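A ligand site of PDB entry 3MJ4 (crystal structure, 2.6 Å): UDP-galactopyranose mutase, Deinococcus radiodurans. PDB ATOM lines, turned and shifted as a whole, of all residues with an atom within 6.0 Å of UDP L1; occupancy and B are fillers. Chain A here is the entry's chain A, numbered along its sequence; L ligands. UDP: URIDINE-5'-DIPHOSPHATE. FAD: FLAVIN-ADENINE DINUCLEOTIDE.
An oxygen (O2A) of UDP L1 lies within hydrogen-bond range of the side-chain hydroxyl (OH) of Tyr 209 (2.7 Å). The side-chain hydroxyl (OG1) of Thr 180 sits at hydrogen-bond distance from an oxygen (O2') of UDP L1. ND2 of Asn 296 is in hydrogen-bond range of O4 of UDP L1, 2.9 Å away. An oxygen (O3A) of UDP L1 lies within hydrogen-bond range of the side-chain hydroxyl (OH) of Tyr 370, 3.0 Å away. The indole nitrogen of Trp 184 sits at hydrogen-bond distance from an oxygen (O3') of UDP L1, at 3.0 Å. N3 of UDP L1 lies within hydrogen-bond range of O of Phe 175, at 3.2 Å. An oxygen (O1A) of UDP L1 is in salt-bridge range of the guanidinium group of Arg 198, 3.2 Å away. O2A of UDP L1 lies within salt-bridge range of NH2 of Arg 305 (3.7 Å). O2P of FAD L2 sits at hydrogen-bond distance from N of Arg 364 (3.1 Å).
OG1 of Thr 180 sits at hydrogen-bond distance from O of Phe 176 (2.8 Å). NE of Arg 305 lies within hydrogen-bond range of OD1 of Asn 296 (3.1 Å). The guanidinium group (NH1) of Arg 198 lies within hydrogen-bond range of the backbone carbonyl oxygen (O) of Tyr 370, at 3.1 Å. OH of Tyr 179 lies within hydrogen-bond range of NE of Arg 305 (3.1 Å). The backbone NH (N) of Tyr 179 sits at hydrogen-bond distance from the backbone carbonyl oxygen (O) of Pro 298, at 3.4 Å. The backbone NH (N) of Ile 122 is in hydrogen-bond range of the backbone carbonyl oxygen (O) of Val 111. The backbone carbonyl oxygen (O) of Ser 159 is in hydrogen-bond range of the side-chain hydroxyl (OG1) of Thr 196, at 2.8 Å.
O of Phe 176 sits close to O2 of UDP L1, 3.5 Å away. Merely in contact with UDP L1: Tyr 179 (3.2 Å), Tyr 335 (3.2 Å), Val 199 (3.7 Å), Ile 122 (3.8 Å), Thr 196 (3.8 Å), Val 195 (3.8 Å) and Gln 183 (3.9 Å). Within 4 Å of UDP L1: Ile 122, Phe 175, Phe 176, Tyr 179, Thr 180, Gln 183, Trp 184, Val 195, Thr 196, Arg 198, Val 199, Tyr 209, Asn 296, Arg 305, Tyr 335 and Tyr 370. The nearest printed residue that does not touch UDP L1 is Arg 364 (4.4 Å).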
ATOM      1  N   VAL A 111     -14.774 -11.199   2.027  1.00  0.00           N
ATOM      2  CA  VAL A 111     -14.825 -10.385   0.822  1.00  0.00           C
ATOM      3  C   VAL A 111     -13.465 -10.348   0.147  1.00  0.00           C
ATOM      4  O   VAL A 111     -12.435 -10.300   0.804  1.00  0.00           O
ATOM      5  CB  VAL A 111     -15.371  -8.949   1.133  1.00  0.00           C
ATOM      6  CG1 VAL A 111     -15.358  -8.054  -0.106  1.00  0.00           C
ATOM      7  CG2 VAL A 111     -16.781  -9.031   1.721  1.00  0.00           C
ATOM      8  N   ALA A 113     -11.259  -8.350  -2.837  1.00  0.00           N
ATOM      9  CA  ALA A 113     -11.273  -7.168  -3.688  1.00  0.00           C
ATOM     10  C   ALA A 113     -10.460  -7.501  -4.909  1.00  0.00           C
ATOM     11  O   ALA A 113      -9.430  -8.162  -4.821  1.00  0.00           O
ATOM     12  CB  ALA A 113     -10.697  -5.963  -2.957  1.00  0.00           C
ATOM     13  N   ILE A 122     -10.097  -8.194   1.750  1.00  0.00           N
ATOM     14  CA  ILE A 122     -10.409  -6.867   2.255  1.00  0.00           C
ATOM     15  C   ILE A 122     -11.350  -7.107   3.427  1.00  0.00           C
ATOM     16  O   ILE A 122     -12.328  -7.844   3.291  1.00  0.00           O
ATOM     17  CB  ILE A 122     -11.104  -6.010   1.165  1.00  0.00           C
ATOM     18  CG1 ILE A 122     -11.509  -4.622   1.687  1.00  0.00           C
ATOM     19  CG2 ILE A 122     -12.324  -6.730   0.635  1.00  0.00           C
ATOM     20  CD1 ILE A 122     -10.364  -3.734   2.084  1.00  0.00           C
ATOM     21  N   SER A 159     -11.995  10.581   5.480  1.00  0.00           N
ATOM     22  CA  SER A 159     -11.887   9.187   5.094  1.00  0.00           C
ATOM     23  C   SER A 159     -10.536   8.864   4.449  1.00  0.00           C
ATOM     24  O   SER A 159     -10.047   7.738   4.560  1.00  0.00           O
ATOM     25  CB  SER A 159     -13.036   8.794   4.177  1.00  0.00           C
ATOM     26  OG  SER A 159     -13.975   8.006   4.861  1.00  0.00           O
ATOM     27  N   PHE A 175      -7.087   0.204  -2.997  1.00  0.00           N
ATOM     28  CA  PHE A 175      -8.205  -0.406  -2.277  1.00  0.00           C
ATOM     29  C   PHE A 175      -9.369   0.568  -1.950  1.00  0.00           C
ATOM     30  O   PHE A 175     -10.527   0.197  -2.067  1.00  0.00           O
ATOM     31  CB  PHE A 175      -7.711  -1.118  -1.004  1.00  0.00           C
ATOM     32  CG  PHE A 175      -6.987  -2.395  -1.279  1.00  0.00           C
ATOM     33  CD1 PHE A 175      -5.603  -2.451  -1.262  1.00  0.00           C
ATOM     34  CD2 PHE A 175      -7.684  -3.544  -1.582  1.00  0.00           C
ATOM     35  CE1 PHE A 175      -4.947  -3.613  -1.536  1.00  0.00           C
ATOM     36  CE2 PHE A 175      -7.028  -4.706  -1.856  1.00  0.00           C
ATOM     37  CZ  PHE A 175      -5.653  -4.743  -1.835  1.00  0.00           C
ATOM     38  N   PHE A 176      -9.045   1.795  -1.563  1.00  0.00           N
ATOM     39  CA  PHE A 176     -10.043   2.722  -1.048  1.00  0.00           C
ATOM     40  C   PHE A 176     -10.478   3.885  -1.961  1.00  0.00           C
ATOM     41  O   PHE A 176     -11.671   4.116  -2.138  1.00  0.00           O
ATOM     42  CB  PHE A 176      -9.602   3.259   0.305  1.00  0.00           C
ATOM     43  CG  PHE A 176      -9.691   2.258   1.390  1.00  0.00           C
ATOM     44  CD1 PHE A 176     -10.855   2.145   2.137  1.00  0.00           C
ATOM     45  CD2 PHE A 176      -8.632   1.415   1.650  1.00  0.00           C
ATOM     46  CE1 PHE A 176     -10.952   1.206   3.131  1.00  0.00           C
ATOM     47  CE2 PHE A 176      -8.729   0.480   2.666  1.00  0.00           C
ATOM     48  CZ  PHE A 176      -9.896   0.375   3.397  1.00  0.00           C
ATOM     49  N   ARG A 177      -9.516   4.603  -2.521  1.00  0.00           N
ATOM     50  CA  ARG A 177      -9.827   5.811  -3.267  1.00  0.00           C
ATOM     51  C   ARG A 177     -10.867   5.530  -4.337  1.00  0.00           C
ATOM     52  O   ARG A 177     -11.945   6.100  -4.321  1.00  0.00           O
ATOM     53  CB  ARG A 177      -8.563   6.432  -3.871  1.00  0.00           C
ATOM     54  CG  ARG A 177      -8.851   7.654  -4.742  1.00  0.00           C
ATOM     55  CD  ARG A 177      -7.595   8.482  -5.033  1.00  0.00           C
ATOM     56  NE  ARG A 177      -6.621   7.732  -5.815  1.00  0.00           N
ATOM     57  CZ  ARG A 177      -6.224   8.053  -7.041  1.00  0.00           C
ATOM     58  NH1 ARG A 177      -6.708   9.135  -7.638  1.00  0.00           N
ATOM     59  NH2 ARG A 177      -5.325   7.294  -7.667  1.00  0.00           N
ATOM     60  N   TYR A 179     -12.824   3.038  -4.950  1.00  0.00           N
ATOM     61  CA  TYR A 179     -14.035   2.367  -4.522  1.00  0.00           C
ATOM     62  C   TYR A 179     -14.969   3.421  -3.945  1.00  0.00           C
ATOM     63  O   TYR A 179     -16.160   3.501  -4.281  1.00  0.00           O
ATOM     64  CB  TYR A 179     -13.713   1.290  -3.465  1.00  0.00           C
ATOM     65  CG  TYR A 179     -14.936   0.513  -3.010  1.00  0.00           C
ATOM     66  CD1 TYR A 179     -15.265  -0.699  -3.596  1.00  0.00           C
ATOM     67  CD2 TYR A 179     -15.778   1.002  -2.019  1.00  0.00           C
ATOM     68  CE1 TYR A 179     -16.390  -1.416  -3.202  1.00  0.00           C
ATOM     69  CE2 TYR A 179     -16.920   0.289  -1.608  1.00  0.00           C
ATOM     70  CZ  TYR A 179     -17.207  -0.921  -2.212  1.00  0.00           C
ATOM     71  OH  TYR A 179     -18.310  -1.649  -1.833  1.00  0.00           O
ATOM     72  N   THR A 180     -14.404   4.217  -3.059  1.00  0.00           N
ATOM     73  CA  THR A 180     -15.102   5.303  -2.414  1.00  0.00           C
ATOM     74  C   THR A 180     -15.574   6.327  -3.418  1.00  0.00           C
ATOM     75  O   THR A 180     -16.763   6.648  -3.439  1.00  0.00           O
ATOM     76  CB  THR A 180     -14.203   5.955  -1.379  1.00  0.00           C
ATOM     77  OG1 THR A 180     -13.746   4.949  -0.475  1.00  0.00           O
ATOM     78  CG2 THR A 180     -14.980   7.031  -0.625  1.00  0.00           C
ATOM     79  N   GLN A 183     -18.630   4.743  -4.877  1.00  0.00           N
ATOM     80  CA  GLN A 183     -19.769   4.400  -4.040  1.00  0.00           C
ATOM     81  C   GLN A 183     -20.511   5.676  -3.600  1.00  0.00           C
ATOM     82  O   GLN A 183     -21.744   5.707  -3.507  1.00  0.00           O
ATOM     83  CB  GLN A 183     -19.267   3.588  -2.837  1.00  0.00           C
ATOM     84  CG  GLN A 183     -20.196   3.517  -1.640  1.00  0.00           C
ATOM     85  CD  GLN A 183     -21.442   2.695  -1.913  1.00  0.00           C
ATOM     86  OE1 GLN A 183     -21.550   2.050  -2.955  1.00  0.00           O
ATOM     87  NE2 GLN A 183     -22.403   2.718  -0.983  1.00  0.00           N
ATOM     88  N   TRP A 184     -19.742   6.726  -3.357  1.00  0.00           N
ATOM     89  CA  TRP A 184     -20.280   7.935  -2.770  1.00  0.00           C
ATOM     90  C   TRP A 184     -20.345   9.086  -3.753  1.00  0.00           C
ATOM     91  O   TRP A 184     -21.033  10.073  -3.517  1.00  0.00           O
ATOM     92  CB  TRP A 184     -19.418   8.322  -1.589  1.00  0.00           C
ATOM     93  CG  TRP A 184     -19.432   7.325  -0.512  1.00  0.00           C
ATOM     94  CD1 TRP A 184     -18.476   6.402  -0.252  1.00  0.00           C
ATOM     95  CD2 TRP A 184     -20.449   7.136   0.470  1.00  0.00           C
ATOM     96  NE1 TRP A 184     -18.811   5.647   0.834  1.00  0.00           N
ATOM     97  CE2 TRP A 184     -20.029   6.085   1.304  1.00  0.00           C
ATOM     98  CE3 TRP A 184     -21.670   7.769   0.739  1.00  0.00           C
ATOM     99  CZ2 TRP A 184     -20.789   5.628   2.376  1.00  0.00           C
ATOM    100  CZ3 TRP A 184     -22.421   7.329   1.798  1.00  0.00           C
ATOM    101  CH2 TRP A 184     -21.982   6.262   2.609  1.00  0.00           C
ATOM    102  N   LEU A 191     -15.253  12.920   2.810  1.00  0.00           N
ATOM    103  CA  LEU A 191     -16.113  12.132   3.679  1.00  0.00           C
ATOM    104  C   LEU A 191     -15.568  12.080   5.080  1.00  0.00           C
ATOM    105  O   LEU A 191     -14.362  12.125   5.295  1.00  0.00           O
ATOM    106  CB  LEU A 191     -16.282  10.711   3.154  1.00  0.00           C
ATOM    107  CG  LEU A 191     -17.016  10.569   1.825  1.00  0.00           C
ATOM    108  CD1 LEU A 191     -16.853   9.175   1.308  1.00  0.00           C
ATOM    109  CD2 LEU A 191     -18.477  10.908   2.012  1.00  0.00           C
ATOM    110  N   VAL A 195     -16.614   6.828   7.840  1.00  0.00           N
ATOM    111  CA  VAL A 195     -16.918   5.968   6.691  1.00  0.00           C
ATOM    112  C   VAL A 195     -15.848   4.858   6.536  1.00  0.00           C
ATOM    113  O   VAL A 195     -16.103   3.685   6.876  1.00  0.00           O
ATOM    114  CB  VAL A 195     -17.040   6.792   5.377  1.00  0.00           C
ATOM    115  CG1 VAL A 195     -17.245   5.874   4.147  1.00  0.00           C
ATOM    116  CG2 VAL A 195     -18.165   7.812   5.494  1.00  0.00           C
ATOM    117  N   THR A 196     -14.655   5.232   6.046  1.00  0.00           N
ATOM    118  CA  THR A 196     -13.630   4.220   5.797  1.00  0.00           C
ATOM    119  C   THR A 196     -13.056   3.593   7.063  1.00  0.00           C
ATOM    120  O   THR A 196     -12.437   2.536   6.977  1.00  0.00           O
ATOM    121  CB  THR A 196     -12.491   4.699   4.885  1.00  0.00           C
ATOM    122  OG1 THR A 196     -11.785   5.787   5.508  1.00  0.00           O
ATOM    123  CG2 THR A 196     -13.007   5.118   3.527  1.00  0.00           C
ATOM    124  N   ARG A 198     -14.783   2.094   9.041  1.00  0.00           N
ATOM    125  CA  ARG A 198     -15.603   0.903   9.195  1.00  0.00           C
ATOM    126  C   ARG A 198     -14.860  -0.348   8.742  1.00  0.00           C
ATOM    127  O   ARG A 198     -15.234  -1.471   9.090  1.00  0.00           O
ATOM    128  CB  ARG A 198     -16.878   1.028   8.386  1.00  0.00           C
ATOM    129  CG  ARG A 198     -17.919   1.893   8.999  1.00  0.00           C
ATOM    130  CD  ARG A 198     -18.978   2.227   7.978  1.00  0.00           C
ATOM    131  NE  ARG A 198     -19.672   1.048   7.484  1.00  0.00           N
ATOM    132  CZ  ARG A 198     -20.816   0.624   7.982  1.00  0.00           C
ATOM    133  NH1 ARG A 198     -21.382   1.301   8.976  1.00  0.00           N
ATOM    134  NH2 ARG A 198     -21.405  -0.450   7.474  1.00  0.00           N
ATOM    135  N   VAL A 199     -13.836  -0.155   7.924  1.00  0.00           N
ATOM    136  CA  VAL A 199     -13.018  -1.259   7.469  1.00  0.00           C
ATOM    137  C   VAL A 199     -11.656  -1.125   8.103  1.00  0.00           C
ATOM    138  O   VAL A 199     -10.868  -0.231   7.772  1.00  0.00           O
ATOM    139  CB  VAL A 199     -12.883  -1.259   5.955  1.00  0.00           C
ATOM    140  CG1 VAL A 199     -12.017  -2.420   5.535  1.00  0.00           C
ATOM    141  CG2 VAL A 199     -14.246  -1.336   5.290  1.00  0.00           C
ATOM    142  N   TYR A 209     -14.786 -10.436   6.890  1.00  0.00           N
ATOM    143  CA  TYR A 209     -15.219  -9.057   6.800  1.00  0.00           C
ATOM    144  C   TYR A 209     -15.507  -8.459   8.185  1.00  0.00           C
ATOM    145  O   TYR A 209     -15.195  -7.302   8.421  1.00  0.00           O
ATOM    146  CB  TYR A 209     -16.401  -8.892   5.848  1.00  0.00           C
ATOM    147  CG  TYR A 209     -16.393  -7.533   5.193  1.00  0.00           C
ATOM    148  CD1 TYR A 209     -15.329  -7.154   4.378  1.00  0.00           C
ATOM    149  CD2 TYR A 209     -17.427  -6.629   5.396  1.00  0.00           C
ATOM    150  CE1 TYR A 209     -15.296  -5.919   3.768  1.00  0.00           C
ATOM    151  CE2 TYR A 209     -17.414  -5.383   4.788  1.00  0.00           C
ATOM    152  CZ  TYR A 209     -16.337  -5.019   3.977  1.00  0.00           C
ATOM    153  OH  TYR A 209     -16.306  -3.760   3.366  1.00  0.00           O
ATOM    154  N   PHE A 210     -16.077  -9.245   9.093  1.00  0.00           N
ATOM    155  CA  PHE A 210     -16.367  -8.771  10.449  1.00  0.00           C
ATOM    156  C   PHE A 210     -15.642  -9.615  11.495  1.00  0.00           C
ATOM    157  O   PHE A 210     -15.406 -10.804  11.284  1.00  0.00           O
ATOM    158  CB  PHE A 210     -17.879  -8.785  10.727  1.00  0.00           C
ATOM    159  CG  PHE A 210     -18.697  -8.210   9.611  1.00  0.00           C
ATOM    160  CD1 PHE A 210     -19.380  -9.041   8.743  1.00  0.00           C
ATOM    161  CD2 PHE A 210     -18.728  -6.843   9.401  1.00  0.00           C
ATOM    162  CE1 PHE A 210     -20.124  -8.510   7.693  1.00  0.00           C
ATOM    163  CE2 PHE A 210     -19.466  -6.307   8.346  1.00  0.00           C
ATOM    164  CZ  PHE A 210     -20.152  -7.138   7.492  1.00  0.00           C
ATOM    165  N   ASN A 296     -15.401  -7.394  -4.354  1.00  0.00           N
ATOM    166  CA  ASN A 296     -15.410  -5.934  -4.514  1.00  0.00           C
ATOM    167  C   ASN A 296     -14.538  -5.518  -5.693  1.00  0.00           C
ATOM    168  O   ASN A 296     -13.492  -6.136  -5.925  1.00  0.00           O
ATOM    169  CB  ASN A 296     -14.897  -5.223  -3.260  1.00  0.00           C
ATOM    170  CG  ASN A 296     -15.951  -5.091  -2.159  1.00  0.00           C
ATOM    171  OD1 ASN A 296     -17.126  -5.396  -2.378  1.00  0.00           O
ATOM    172  ND2 ASN A 296     -15.533  -4.649  -0.975  1.00  0.00           N
ATOM    173  N   PRO A 298     -12.773  -2.148  -6.709  1.00  0.00           N
ATOM    174  CA  PRO A 298     -12.402  -0.754  -6.480  1.00  0.00           C
ATOM    175  C   PRO A 298     -11.888  -0.013  -7.728  1.00  0.00           C
ATOM    176  O   PRO A 298     -11.930   1.224  -7.741  1.00  0.00           O
ATOM    177  CB  PRO A 298     -11.260  -0.870  -5.465  1.00  0.00           C
ATOM    178  CG  PRO A 298     -11.445  -2.208  -4.847  1.00  0.00           C
ATOM    179  CD  PRO A 298     -11.904  -3.064  -5.959  1.00  0.00           C
ATOM    180  N   ARG A 305     -19.490  -3.952  -6.528  1.00  0.00           N
ATOM    181  CA  ARG A 305     -19.374  -5.311  -6.007  1.00  0.00           C
ATOM    182  C   ARG A 305     -20.422  -6.255  -6.582  1.00  0.00           C
ATOM    183  O   ARG A 305     -21.484  -5.818  -7.031  1.00  0.00           O
ATOM    184  CB  ARG A 305     -19.465  -5.300  -4.481  1.00  0.00           C
ATOM    185  CG  ARG A 305     -20.622  -4.469  -3.959  1.00  0.00           C
ATOM    186  CD  ARG A 305     -20.967  -4.761  -2.504  1.00  0.00           C
ATOM    187  NE  ARG A 305     -19.930  -4.320  -1.567  1.00  0.00           N
ATOM    188  NH1 ARG A 305     -20.476  -5.910   0.008  1.00  0.00           N
ATOM    189  NH2 ARG A 305     -18.739  -4.442   0.432  1.00  0.00           N
ATOM    190  N   TYR A 335     -28.046   5.253   2.097  1.00  0.00           N
ATOM    191  CA  TYR A 335     -27.012   5.621   3.062  1.00  0.00           C
ATOM    192  C   TYR A 335     -27.082   7.096   3.341  1.00  0.00           C
ATOM    193  O   TYR A 335     -27.291   7.896   2.436  1.00  0.00           O
ATOM    194  CB  TYR A 335     -25.604   5.352   2.521  1.00  0.00           C
ATOM    195  CG  TYR A 335     -25.333   3.980   1.961  1.00  0.00           C
ATOM    196  CD1 TYR A 335     -25.859   3.600   0.738  1.00  0.00           C
ATOM    197  CD2 TYR A 335     -24.489   3.089   2.623  1.00  0.00           C
ATOM    198  CE1 TYR A 335     -25.587   2.352   0.207  1.00  0.00           C
ATOM    199  CE2 TYR A 335     -24.204   1.842   2.110  1.00  0.00           C
ATOM    200  CZ  TYR A 335     -24.752   1.486   0.895  1.00  0.00           C
ATOM    201  OH  TYR A 335     -24.493   0.241   0.367  1.00  0.00           O
ATOM    202  N   ARG A 364     -31.920   4.241  10.731  1.00  0.00           N
ATOM    203  CA  ARG A 364     -30.820   4.717   9.934  1.00  0.00           C
ATOM    204  C   ARG A 364     -31.219   5.996   9.184  1.00  0.00           C
ATOM    205  O   ARG A 364     -30.543   7.017   9.276  1.00  0.00           O
ATOM    206  CB  ARG A 364     -30.422   3.609   8.974  1.00  0.00           C
ATOM    207  CG  ARG A 364     -29.121   3.787   8.222  1.00  0.00           C
ATOM    208  CD  ARG A 364     -28.957   2.641   7.269  1.00  0.00           C
ATOM    209  NE  ARG A 364     -27.565   2.420   6.877  1.00  0.00           N
ATOM    210  CZ  ARG A 364     -27.209   1.995   5.673  1.00  0.00           C
ATOM    211  NH1 ARG A 364     -28.156   1.749   4.776  1.00  0.00           N
ATOM    212  NH2 ARG A 364     -25.939   1.801   5.364  1.00  0.00           N
ATOM    213  N   TYR A 370     -25.146   6.062   9.926  1.00  0.00           N
ATOM    214  CA  TYR A 370     -24.627   4.952   9.112  1.00  0.00           C
ATOM    215  C   TYR A 370     -24.629   3.659   9.923  1.00  0.00           C
ATOM    216  O   TYR A 370     -23.570   3.107  10.217  1.00  0.00           O
ATOM    217  CB  TYR A 370     -23.189   5.273   8.686  1.00  0.00           C
ATOM    218  CG  TYR A 370     -22.642   4.500   7.509  1.00  0.00           C
ATOM    219  CD1 TYR A 370     -23.233   3.313   7.075  1.00  0.00           C
ATOM    220  CD2 TYR A 370     -21.500   4.937   6.849  1.00  0.00           C
ATOM    221  CE1 TYR A 370     -22.712   2.606   5.994  1.00  0.00           C
ATOM    222  CE2 TYR A 370     -20.957   4.223   5.775  1.00  0.00           C
ATOM    223  CZ  TYR A 370     -21.572   3.072   5.355  1.00  0.00           C
ATOM    224  OH  TYR A 370     -21.043   2.386   4.283  1.00  0.00           O
HETATM  225  N1  UDP L   1     -14.504   0.653   1.228  1.00  0.00           N
HETATM  226  C2  UDP L   1     -13.547   0.719   0.252  1.00  0.00           C
HETATM  227  N3  UDP L   1     -13.200  -0.398  -0.464  1.00  0.00           N
HETATM  228  C4  UDP L   1     -13.828  -1.591  -0.181  1.00  0.00           C
HETATM  229  C5  UDP L   1     -14.798  -1.637   0.813  1.00  0.00           C
HETATM  230  C6  UDP L   1     -14.910  -0.559   1.686  1.00  0.00           C
HETATM  231  O2  UDP L   1     -13.017   1.801   0.044  1.00  0.00           O
HETATM  232  O4  UDP L   1     -13.537  -2.603  -0.811  1.00  0.00           O
HETATM  233  C1' UDP L   1     -14.821   1.878   1.922  1.00  0.00           C
HETATM  234  C2' UDP L   1     -15.919   2.525   1.109  1.00  0.00           C
HETATM  235  O2' UDP L   1     -15.792   3.926   1.180  1.00  0.00           O
HETATM  236  C3' UDP L   1     -17.154   2.048   1.852  1.00  0.00           C
HETATM  237  C4' UDP L   1     -16.669   2.059   3.280  1.00  0.00           C
HETATM  238  O4' UDP L   1     -15.354   1.562   3.177  1.00  0.00           O
HETATM  239  O3' UDP L   1     -18.280   2.861   1.684  1.00  0.00           O
HETATM  240  C5' UDP L   1     -17.510   1.192   4.184  1.00  0.00           C
HETATM  241  O5' UDP L   1     -17.863   0.025   3.487  1.00  0.00           O
HETATM  242  PA  UDP L   1     -18.724  -1.097   4.248  1.00  0.00           P
HETATM  243  O1A UDP L   1     -18.281  -1.212   5.664  1.00  0.00           O
HETATM  244  O2A UDP L   1     -18.667  -2.391   3.515  1.00  0.00           O
HETATM  245  O3A UDP L   1     -20.205  -0.452   4.265  1.00  0.00           O
HETATM  246  PB  UDP L   1     -21.309  -0.893   3.163  1.00  0.00           P
HETATM  247  O1B UDP L   1     -20.939  -0.160   1.917  1.00  0.00           O
HETATM  248  O2B UDP L   1     -22.702  -0.573   3.598  1.00  0.00           O
HETATM  249  O3B UDP L   1     -21.215  -2.358   2.905  1.00  0.00           O
HETATM  250  PA  FAD L   2     -35.140   0.633   6.502  1.00  0.00           P
HETATM  251  O1A FAD L   2     -34.639   1.456   5.323  1.00  0.00           O
HETATM  252  O2A FAD L   2     -34.887  -0.835   6.254  1.00  0.00           O
HETATM  253  O5B FAD L   2     -36.715   0.851   6.716  1.00  0.00           O
HETATM  254  C5B FAD L   2     -37.365   2.089   6.571  1.00  0.00           C
HETATM  255  C4B FAD L   2     -38.662   1.814   5.831  1.00  0.00           C
HETATM  256  O4B FAD L   2     -39.595   2.890   5.937  1.00  0.00           O
HETATM  257  C3B FAD L   2     -38.427   1.562   4.341  1.00  0.00           C
HETATM  258  O3B FAD L   2     -38.803   0.225   4.095  1.00  0.00           O
HETATM  259  C2B FAD L   2     -39.341   2.571   3.643  1.00  0.00           C
HETATM  260  O2B FAD L   2     -40.018   2.021   2.525  1.00  0.00           O
HETATM  261  C1B FAD L   2     -40.328   2.972   4.740  1.00  0.00           C
HETATM  262  N9A FAD L   2     -40.819   4.342   4.581  1.00  0.00           N
HETATM  263  C8A FAD L   2     -40.051   5.469   4.434  1.00  0.00           C
HETATM  264  N7A FAD L   2     -40.868   6.530   4.309  1.00  0.00           N
HETATM  265  C5A FAD L   2     -42.161   6.111   4.380  1.00  0.00           C
HETATM  266  C6A FAD L   2     -43.377   6.797   4.305  1.00  0.00           C
HETATM  267  N6A FAD L   2     -43.413   7.855   3.492  1.00  0.00           N
HETATM  268  N1A FAD L   2     -44.551   6.084   4.428  1.00  0.00           N
HETATM  269  C2A FAD L   2     -44.519   4.707   4.594  1.00  0.00           C
HETATM  270  N3A FAD L   2     -43.311   4.036   4.652  1.00  0.00           N
HETATM  271  C4A FAD L   2     -42.144   4.725   4.557  1.00  0.00           C
HETATM  272  N1  FAD L   2     -26.527  -3.898   7.662  1.00  0.00           N
HETATM  273  C2  FAD L   2     -25.843  -4.939   8.264  1.00  0.00           C
HETATM  274  O2  FAD L   2     -25.803  -5.050   9.491  1.00  0.00           O
HETATM  275  N3  FAD L   2     -25.175  -5.870   7.499  1.00  0.00           N
HETATM  276  C4  FAD L   2     -25.180  -5.777   6.136  1.00  0.00           C
HETATM  277  O4  FAD L   2     -24.572  -6.640   5.478  1.00  0.00           O
HETATM  278  C4X FAD L   2     -25.867  -4.728   5.518  1.00  0.00           C
HETATM  279  N5  FAD L   2     -25.895  -4.628   4.148  1.00  0.00           N
HETATM  280  C5X FAD L   2     -26.567  -3.607   3.528  1.00  0.00           C
HETATM  281  C6  FAD L   2     -26.546  -3.537   2.142  1.00  0.00           C
HETATM  282  C7  FAD L   2     -27.223  -2.518   1.476  1.00  0.00           C
HETATM  283  C7M FAD L   2     -27.196  -2.483  -0.025  1.00  0.00           C
HETATM  284  C8  FAD L   2     -27.918  -1.559   2.226  1.00  0.00           C
HETATM  285  C8M FAD L   2     -28.642  -0.450   1.494  1.00  0.00           C
HETATM  286  C9  FAD L   2     -27.932  -1.620   3.628  1.00  0.00           C
HETATM  287  C9A FAD L   2     -27.252  -2.652   4.287  1.00  0.00           C
HETATM  288  N10 FAD L   2     -27.239  -2.744   5.683  1.00  0.00           N
HETATM  289  C10 FAD L   2     -26.537  -3.784   6.290  1.00  0.00           C
HETATM  290  C1' FAD L   2     -27.938  -1.739   6.541  1.00  0.00           C
HETATM  291  C2' FAD L   2     -29.300  -2.217   7.035  1.00  0.00           C
HETATM  292  O2' FAD L   2     -30.151  -2.446   5.945  1.00  0.00           O
HETATM  293  C3' FAD L   2     -29.882  -1.138   7.927  1.00  0.00           C
HETATM  294  O3' FAD L   2     -29.188  -1.140   9.157  1.00  0.00           O
HETATM  295  C4' FAD L   2     -31.374  -1.337   8.116  1.00  0.00           C
HETATM  296  O4' FAD L   2     -32.020  -0.938   6.941  1.00  0.00           O
HETATM  297  C5' FAD L   2     -31.959  -0.458   9.215  1.00  0.00           C
HETATM  298  O5' FAD L   2     -33.364  -0.604   9.171  1.00  0.00           O
HETATM  299  P   FAD L   2     -34.307   0.697   9.280  1.00  0.00           P
HETATM  300  O1P FAD L   2     -35.637   0.304   9.871  1.00  0.00           O
HETATM  301  O2P FAD L   2     -33.623   1.720  10.140  1.00  0.00           O
HETATM  302  O3P FAD L   2     -34.431   1.275   7.798  1.00  0.00           O
